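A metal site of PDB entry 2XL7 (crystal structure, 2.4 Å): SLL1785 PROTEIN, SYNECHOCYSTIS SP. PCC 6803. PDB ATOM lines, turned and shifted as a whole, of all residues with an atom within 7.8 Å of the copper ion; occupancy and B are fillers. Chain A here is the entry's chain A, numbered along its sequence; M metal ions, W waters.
The side-chain amide oxygen of Gln 191 sits close to a ring nitrogen (ND1) of His 59. The backbone carbonyl oxygen of Met 57 sits at hydrogen-bond distance from a ring nitrogen (ND1) of His 59, 3.1 Å away. The side-chain carboxylate (OE2) of Glu 66 sits at hydrogen-bond distance from the indole nitrogen (NE1) of Trp 136 (2.8 Å). The backbone carbonyl oxygen of Glu 66 is in hydrogen-bond range of the backbone NH of Ser 114 (2.8 Å). ND1 of His 120 lies within hydrogen-bond range of OG of Ser 114, at 2.8 Å.
NE2 of His 59 is bound to the copper ion, 2.0 Å away. The copper ion is bound by OE1 of Glu 66, 2.0 Å away. A ring nitrogen (NE2) of His 61 is bound to the copper ion, 2.1 Å away. NE2 of His 120 binds the copper ion, 2.2 Å away. The copper ion has four donor atoms within binding distance.
Within 4 Å of the copper ion: His 59, His 61, Glu 66 and His 120.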
ATOM      1  N   PRO A  56      35.067  -5.318 -22.274  1.00  0.00           N
ATOM      2  CA  PRO A  56      34.422  -4.295 -21.449  1.00  0.00           C
ATOM      3  C   PRO A  56      35.262  -3.933 -20.225  1.00  0.00           C
ATOM      4  O   PRO A  56      36.011  -4.787 -19.744  1.00  0.00           O
ATOM      5  CB  PRO A  56      33.127  -5.013 -21.012  1.00  0.00           C
ATOM      6  CG  PRO A  56      33.531  -6.443 -20.920  1.00  0.00           C
ATOM      7  CD  PRO A  56      34.495  -6.660 -22.054  1.00  0.00           C
ATOM      8  N   MET A  57      35.128  -2.685 -19.760  1.00  0.00           N
ATOM      9  CA  MET A  57      35.705  -2.207 -18.498  1.00  0.00           C
ATOM     10  C   MET A  57      35.057  -2.951 -17.315  1.00  0.00           C
ATOM     11  O   MET A  57      33.939  -3.483 -17.451  1.00  0.00           O
ATOM     12  CB  MET A  57      35.469  -0.693 -18.312  1.00  0.00           C
ATOM     13  CG  MET A  57      35.784   0.201 -19.512  1.00  0.00           C
ATOM     14  SD  MET A  57      37.650   0.075 -19.975  1.00  0.00           S
ATOM     15  CE  MET A  57      37.532   0.911 -21.763  1.00  0.00           C
ATOM     16  N   PRO A  58      35.736  -2.989 -16.155  1.00  0.00           N
ATOM     17  CA  PRO A  58      35.187  -3.663 -14.978  1.00  0.00           C
ATOM     18  C   PRO A  58      33.736  -3.281 -14.715  1.00  0.00           C
ATOM     19  O   PRO A  58      33.379  -2.118 -14.827  1.00  0.00           O
ATOM     20  CB  PRO A  58      36.094  -3.177 -13.854  1.00  0.00           C
ATOM     21  CG  PRO A  58      37.410  -2.973 -14.513  1.00  0.00           C
ATOM     22  CD  PRO A  58      37.062  -2.394 -15.858  1.00  0.00           C
ATOM     23  N   HIS A  59      32.924  -4.278 -14.396  1.00  0.00           N
ATOM     24  CA  HIS A  59      31.507  -4.060 -14.149  1.00  0.00           C
ATOM     25  C   HIS A  59      30.951  -5.108 -13.210  1.00  0.00           C
ATOM     26  O   HIS A  59      31.613  -6.126 -12.976  1.00  0.00           O
ATOM     27  CB  HIS A  59      30.714  -4.001 -15.463  1.00  0.00           C
ATOM     28  CG  HIS A  59      30.721  -5.277 -16.239  1.00  0.00           C
ATOM     29  ND1 HIS A  59      31.638  -5.534 -17.235  1.00  0.00           N
ATOM     30  CD2 HIS A  59      29.902  -6.349 -16.203  1.00  0.00           C
ATOM     31  CE1 HIS A  59      31.392  -6.717 -17.765  1.00  0.00           C
ATOM     32  NE2 HIS A  59      30.345  -7.236 -17.164  1.00  0.00           N
ATOM     33  N   ILE A  60      29.765  -4.854 -12.647  1.00  0.00           N
ATOM     34  CA  ILE A  60      29.126  -5.760 -11.703  1.00  0.00           C
ATOM     35  C   ILE A  60      27.680  -6.023 -12.106  1.00  0.00           C
ATOM     36  O   ILE A  60      26.939  -5.084 -12.459  1.00  0.00           O
ATOM     37  CB  ILE A  60      29.156  -5.188 -10.262  1.00  0.00           C
ATOM     38  CG1 ILE A  60      30.582  -4.891  -9.811  1.00  0.00           C
ATOM     39  CG2 ILE A  60      28.477  -6.147  -9.271  1.00  0.00           C
ATOM     40  CD1 ILE A  60      30.657  -3.826  -8.751  1.00  0.00           C
ATOM     41  N   HIS A  61      27.259  -7.287 -12.041  1.00  0.00           N
ATOM     42  CA  HIS A  61      25.878  -7.671 -12.386  1.00  0.00           C
ATOM     43  C   HIS A  61      24.985  -7.853 -11.168  1.00  0.00           C
ATOM     44  O   HIS A  61      25.403  -8.370 -10.137  1.00  0.00           O
ATOM     45  CB  HIS A  61      25.844  -8.946 -13.228  1.00  0.00           C
ATOM     46  CG  HIS A  61      26.536  -8.834 -14.548  1.00  0.00           C
ATOM     47  ND1 HIS A  61      25.889  -8.404 -15.688  1.00  0.00           N
ATOM     48  CD2 HIS A  61      27.818  -9.099 -14.912  1.00  0.00           C
ATOM     49  CE1 HIS A  61      26.746  -8.409 -16.703  1.00  0.00           C
ATOM     50  NE2 HIS A  61      27.921  -8.814 -16.258  1.00  0.00           N
ATOM     51  N   ILE A  64      21.924 -11.059 -13.342  1.00  0.00           N
ATOM     52  CA  ILE A  64      22.399 -12.290 -14.013  1.00  0.00           C
ATOM     53  C   ILE A  64      23.651 -12.907 -13.399  1.00  0.00           C
ATOM     54  O   ILE A  64      24.391 -12.240 -12.672  1.00  0.00           O
ATOM     55  CB  ILE A  64      22.652 -12.101 -15.552  1.00  0.00           C
ATOM     56  CG1 ILE A  64      23.822 -11.143 -15.829  1.00  0.00           C
ATOM     57  CG2 ILE A  64      21.368 -11.701 -16.279  1.00  0.00           C
ATOM     58  CD1 ILE A  64      25.197 -11.806 -15.843  1.00  0.00           C
ATOM     59  N   ASN A  65      23.863 -14.188 -13.694  1.00  0.00           N
ATOM     60  CA  ASN A  65      25.127 -14.879 -13.468  1.00  0.00           C
ATOM     61  C   ASN A  65      25.739 -15.117 -14.845  1.00  0.00           C
ATOM     62  O   ASN A  65      25.019 -15.418 -15.800  1.00  0.00           O
ATOM     63  CB  ASN A  65      24.910 -16.216 -12.763  1.00  0.00           C
ATOM     64  CG  ASN A  65      24.219 -16.065 -11.430  1.00  0.00           C
ATOM     65  OD1 ASN A  65      24.750 -15.441 -10.503  1.00  0.00           O
ATOM     66  ND2 ASN A  65      23.045 -16.647 -11.307  1.00  0.00           N
ATOM     67  N   GLU A  66      27.071 -14.987 -14.944  1.00  0.00           N
ATOM     68  CA  GLU A  66      27.734 -14.975 -16.240  1.00  0.00           C
ATOM     69  C   GLU A  66      28.730 -16.115 -16.373  1.00  0.00           C
ATOM     70  O   GLU A  66      29.435 -16.411 -15.428  1.00  0.00           O
ATOM     71  CB  GLU A  66      28.456 -13.622 -16.455  1.00  0.00           C
ATOM     72  CG  GLU A  66      29.032 -13.431 -17.853  1.00  0.00           C
ATOM     73  CD  GLU A  66      29.362 -11.966 -18.164  1.00  0.00           C
ATOM     74  OE1 GLU A  66      29.319 -11.125 -17.246  1.00  0.00           O
ATOM     75  OE2 GLU A  66      29.674 -11.649 -19.329  1.00  0.00           O
ATOM     76  N   TRP A  67      28.781 -16.710 -17.559  1.00  0.00           N
ATOM     77  CA  TRP A  67      29.812 -17.667 -17.909  1.00  0.00           C
ATOM     78  C   TRP A  67      30.637 -17.102 -19.061  1.00  0.00           C
ATOM     79  O   TRP A  67      30.058 -16.517 -20.002  1.00  0.00           O
ATOM     80  CB  TRP A  67      29.219 -19.002 -18.379  1.00  0.00           C
ATOM     81  CG  TRP A  67      28.600 -19.877 -17.334  1.00  0.00           C
ATOM     82  CD1 TRP A  67      29.092 -21.070 -16.872  1.00  0.00           C
ATOM     83  CD2 TRP A  67      27.318 -19.710 -16.696  1.00  0.00           C
ATOM     84  NE1 TRP A  67      28.225 -21.628 -15.955  1.00  0.00           N
ATOM     85  CE2 TRP A  67      27.123 -20.815 -15.836  1.00  0.00           C
ATOM     86  CE3 TRP A  67      26.335 -18.716 -16.755  1.00  0.00           C
ATOM     87  CZ2 TRP A  67      25.985 -20.950 -15.022  1.00  0.00           C
ATOM     88  CZ3 TRP A  67      25.196 -18.852 -15.954  1.00  0.00           C
ATOM     89  CH2 TRP A  67      25.036 -19.962 -15.105  1.00  0.00           C
ATOM     90  N   PHE A  68      31.955 -17.273 -18.990  1.00  0.00           N
ATOM     91  CA  PHE A  68      32.854 -16.907 -20.085  1.00  0.00           C
ATOM     92  C   PHE A  68      33.513 -18.178 -20.564  1.00  0.00           C
ATOM     93  O   PHE A  68      34.057 -18.952 -19.771  1.00  0.00           O
ATOM     94  CB  PHE A  68      33.982 -15.981 -19.606  1.00  0.00           C
ATOM     95  CG  PHE A  68      33.498 -14.724 -18.952  1.00  0.00           C
ATOM     96  CD1 PHE A  68      33.320 -13.565 -19.702  1.00  0.00           C
ATOM     97  CD2 PHE A  68      33.291 -14.685 -17.582  1.00  0.00           C
ATOM     98  CE1 PHE A  68      32.892 -12.377 -19.087  1.00  0.00           C
ATOM     99  CE2 PHE A  68      32.885 -13.506 -16.947  1.00  0.00           C
ATOM    100  CZ  PHE A  68      32.694 -12.348 -17.701  1.00  0.00           C
ATOM    101  N   SER A 114      31.099 -16.611 -13.232  1.00  0.00           N
ATOM    102  CA  SER A 114      31.099 -15.395 -12.431  1.00  0.00           C
ATOM    103  C   SER A 114      29.692 -15.003 -11.936  1.00  0.00           C
ATOM    104  O   SER A 114      28.918 -14.385 -12.679  1.00  0.00           O
ATOM    105  CB  SER A 114      31.763 -14.265 -13.227  1.00  0.00           C
ATOM    106  OG  SER A 114      31.907 -13.109 -12.422  1.00  0.00           O
ATOM    107  N   TYR A 118      29.989 -10.044  -8.155  1.00  0.00           N
ATOM    108  CA  TYR A 118      31.433  -9.998  -8.379  1.00  0.00           C
ATOM    109  C   TYR A 118      31.767  -8.941  -9.410  1.00  0.00           C
ATOM    110  O   TYR A 118      30.981  -8.702 -10.339  1.00  0.00           O
ATOM    111  CB  TYR A 118      31.929 -11.349  -8.884  1.00  0.00           C
ATOM    112  CG  TYR A 118      32.122 -12.364  -7.801  1.00  0.00           C
ATOM    113  CD1 TYR A 118      33.309 -12.421  -7.070  1.00  0.00           C
ATOM    114  CD2 TYR A 118      31.109 -13.268  -7.486  1.00  0.00           C
ATOM    115  CE1 TYR A 118      33.496 -13.365  -6.072  1.00  0.00           C
ATOM    116  CE2 TYR A 118      31.288 -14.217  -6.486  1.00  0.00           C
ATOM    117  CZ  TYR A 118      32.486 -14.245  -5.784  1.00  0.00           C
ATOM    118  OH  TYR A 118      32.682 -15.167  -4.793  1.00  0.00           O
ATOM    119  N   MET A 119      32.923  -8.309  -9.263  1.00  0.00           N
ATOM    120  CA  MET A 119      33.382  -7.372 -10.274  1.00  0.00           C
ATOM    121  C   MET A 119      34.208  -8.125 -11.289  1.00  0.00           C
ATOM    122  O   MET A 119      35.081  -8.912 -10.913  1.00  0.00           O
ATOM    123  CB  MET A 119      34.223  -6.258  -9.644  1.00  0.00           C
ATOM    124  CG  MET A 119      34.607  -5.165 -10.631  1.00  0.00           C
ATOM    125  SD  MET A 119      35.776  -3.832  -9.889  1.00  0.00           S
ATOM    126  CE  MET A 119      34.759  -3.347  -8.356  1.00  0.00           C
ATOM    127  N   HIS A 120      33.967  -7.874 -12.571  1.00  0.00           N
ATOM    128  CA  HIS A 120      34.797  -8.484 -13.608  1.00  0.00           C
ATOM    129  C   HIS A 120      34.892  -7.653 -14.879  1.00  0.00           C
ATOM    130  O   HIS A 120      34.241  -6.635 -15.028  1.00  0.00           O
ATOM    131  CB  HIS A 120      34.332  -9.926 -13.930  1.00  0.00           C
ATOM    132  CG  HIS A 120      32.942 -10.010 -14.486  1.00  0.00           C
ATOM    133  ND1 HIS A 120      31.960 -10.793 -13.916  1.00  0.00           N
ATOM    134  CD2 HIS A 120      32.370  -9.417 -15.561  1.00  0.00           C
ATOM    135  CE1 HIS A 120      30.843 -10.680 -14.618  1.00  0.00           C
ATOM    136  NE2 HIS A 120      31.060  -9.853 -15.622  1.00  0.00           N
ATOM    137  N   GLY A 121      35.740  -8.122 -15.801  1.00  0.00           N
ATOM    138  CA  GLY A 121      35.902  -7.548 -17.126  1.00  0.00           C
ATOM    139  C   GLY A 121      36.863  -8.438 -17.857  1.00  0.00           C
ATOM    140  O   GLY A 121      37.264  -9.489 -17.330  1.00  0.00           O
ATOM    141  N   PHE A 122      37.231  -8.057 -19.073  1.00  0.00           N
ATOM    142  CA  PHE A 122      38.261  -8.788 -19.817  1.00  0.00           C
ATOM    143  C   PHE A 122      38.774  -7.940 -20.957  1.00  0.00           C
ATOM    144  O   PHE A 122      38.150  -6.962 -21.321  1.00  0.00           O
ATOM    145  CB  PHE A 122      37.741 -10.135 -20.354  1.00  0.00           C
ATOM    146  CG  PHE A 122      36.777  -9.997 -21.498  1.00  0.00           C
ATOM    147  CD1 PHE A 122      37.236  -9.830 -22.809  1.00  0.00           C
ATOM    148  CD2 PHE A 122      35.402 -10.031 -21.258  1.00  0.00           C
ATOM    149  CE1 PHE A 122      36.356  -9.688 -23.857  1.00  0.00           C
ATOM    150  CE2 PHE A 122      34.493  -9.883 -22.311  1.00  0.00           C
ATOM    151  CZ  PHE A 122      34.962  -9.708 -23.610  1.00  0.00           C
ATOM    152  N   PHE A 134      29.633 -15.985 -24.291  1.00  0.00           N
ATOM    153  CA  PHE A 134      29.065 -15.588 -23.018  1.00  0.00           C
ATOM    154  C   PHE A 134      27.714 -16.234 -22.850  1.00  0.00           C
ATOM    155  O   PHE A 134      26.952 -16.369 -23.810  1.00  0.00           O
ATOM    156  CB  PHE A 134      28.768 -14.092 -22.965  1.00  0.00           C
ATOM    157  CG  PHE A 134      29.902 -13.213 -23.373  1.00  0.00           C
ATOM    158  CD1 PHE A 134      30.742 -12.668 -22.411  1.00  0.00           C
ATOM    159  CD2 PHE A 134      30.099 -12.861 -24.710  1.00  0.00           C
ATOM    160  CE1 PHE A 134      31.790 -11.815 -22.794  1.00  0.00           C
ATOM    161  CE2 PHE A 134      31.117 -12.018 -25.094  1.00  0.00           C
ATOM    162  CZ  PHE A 134      31.976 -11.488 -24.139  1.00  0.00           C
ATOM    163  N   TRP A 136      24.554 -15.372 -20.162  1.00  0.00           N
ATOM    164  CA  TRP A 136      24.057 -14.602 -19.039  1.00  0.00           C
ATOM    165  C   TRP A 136      22.707 -15.149 -18.650  1.00  0.00           C
ATOM    166  O   TRP A 136      21.717 -14.958 -19.371  1.00  0.00           O
ATOM    167  CB  TRP A 136      23.902 -13.127 -19.396  1.00  0.00           C
ATOM    168  CG  TRP A 136      25.098 -12.466 -20.018  1.00  0.00           C
ATOM    169  CD1 TRP A 136      26.115 -11.850 -19.351  1.00  0.00           C
ATOM    170  CD2 TRP A 136      25.372 -12.290 -21.419  1.00  0.00           C
ATOM    171  NE1 TRP A 136      27.011 -11.305 -20.240  1.00  0.00           N
ATOM    172  CE2 TRP A 136      26.585 -11.564 -21.517  1.00  0.00           C
ATOM    173  CE3 TRP A 136      24.722 -12.672 -22.602  1.00  0.00           C
ATOM    174  CZ2 TRP A 136      27.159 -11.215 -22.750  1.00  0.00           C
ATOM    175  CZ3 TRP A 136      25.285 -12.321 -23.826  1.00  0.00           C
ATOM    176  CH2 TRP A 136      26.503 -11.603 -23.879  1.00  0.00           C
ATOM    177  N   MET A 152      20.181  -8.847 -20.486  1.00  0.00           N
ATOM    178  CA  MET A 152      21.459  -8.595 -21.184  1.00  0.00           C
ATOM    179  C   MET A 152      21.352  -8.378 -22.705  1.00  0.00           C
ATOM    180  O   MET A 152      22.002  -7.464 -23.237  1.00  0.00           O
ATOM    181  CB  MET A 152      22.513  -9.641 -20.842  1.00  0.00           C
ATOM    182  CG  MET A 152      22.898  -9.647 -19.368  1.00  0.00           C
ATOM    183  SD  MET A 152      23.609  -7.930 -18.765  1.00  0.00           S
ATOM    184  CE  MET A 152      25.178  -7.855 -19.931  1.00  0.00           C
ATOM    185  N   PHE A 156      22.449  -4.863 -24.767  1.00  0.00           N
ATOM    186  CA  PHE A 156      23.351  -4.742 -25.908  1.00  0.00           C
ATOM    187  C   PHE A 156      22.600  -4.182 -27.102  1.00  0.00           C
ATOM    188  O   PHE A 156      23.120  -3.353 -27.817  1.00  0.00           O
ATOM    189  CB  PHE A 156      24.049  -6.059 -26.253  1.00  0.00           C
ATOM    190  CG  PHE A 156      24.996  -6.527 -25.194  1.00  0.00           C
ATOM    191  CD1 PHE A 156      26.132  -5.773 -24.893  1.00  0.00           C
ATOM    192  CD2 PHE A 156      24.741  -7.692 -24.466  1.00  0.00           C
ATOM    193  CE1 PHE A 156      27.023  -6.173 -23.889  1.00  0.00           C
ATOM    194  CE2 PHE A 156      25.607  -8.106 -23.456  1.00  0.00           C
ATOM    195  CZ  PHE A 156      26.760  -7.353 -23.179  1.00  0.00           C
ATOM    196  N   ILE A 189      23.320  -3.597 -14.329  1.00  0.00           N
ATOM    197  CA  ILE A 189      24.780  -3.567 -14.399  1.00  0.00           C
ATOM    198  C   ILE A 189      25.284  -2.224 -13.880  1.00  0.00           C
ATOM    199  O   ILE A 189      24.766  -1.173 -14.267  1.00  0.00           O
ATOM    200  CB  ILE A 189      25.290  -3.710 -15.852  1.00  0.00           C
ATOM    201  CG1 ILE A 189      24.438  -4.712 -16.634  1.00  0.00           C
ATOM    202  CG2 ILE A 189      26.800  -4.047 -15.886  1.00  0.00           C
ATOM    203  CD1 ILE A 189      24.536  -4.543 -18.168  1.00  0.00           C
ATOM    204  N   GLN A 191      28.336  -0.370 -14.643  1.00  0.00           N
ATOM    205  CA  GLN A 191      29.398  -0.438 -15.654  1.00  0.00           C
ATOM    206  C   GLN A 191      30.320   0.801 -15.600  1.00  0.00           C
ATOM    207  O   GLN A 191      29.872   1.952 -15.768  1.00  0.00           O
ATOM    208  CB  GLN A 191      28.773  -0.616 -17.048  1.00  0.00           C
ATOM    209  CG  GLN A 191      29.761  -0.545 -18.207  1.00  0.00           C
ATOM    210  CD  GLN A 191      30.738  -1.701 -18.218  1.00  0.00           C
ATOM    211  OE1 GLN A 191      30.358  -2.849 -18.414  1.00  0.00           O
ATOM    212  NE2 GLN A 191      32.028  -1.390 -18.020  1.00  0.00           N
HETATM  213 CU    CU M   1      29.712  -9.136 -17.262  1.00  0.00          CU
HETATM  214  O   HOH W   1      31.318  -9.583 -19.866  1.00  0.00           O
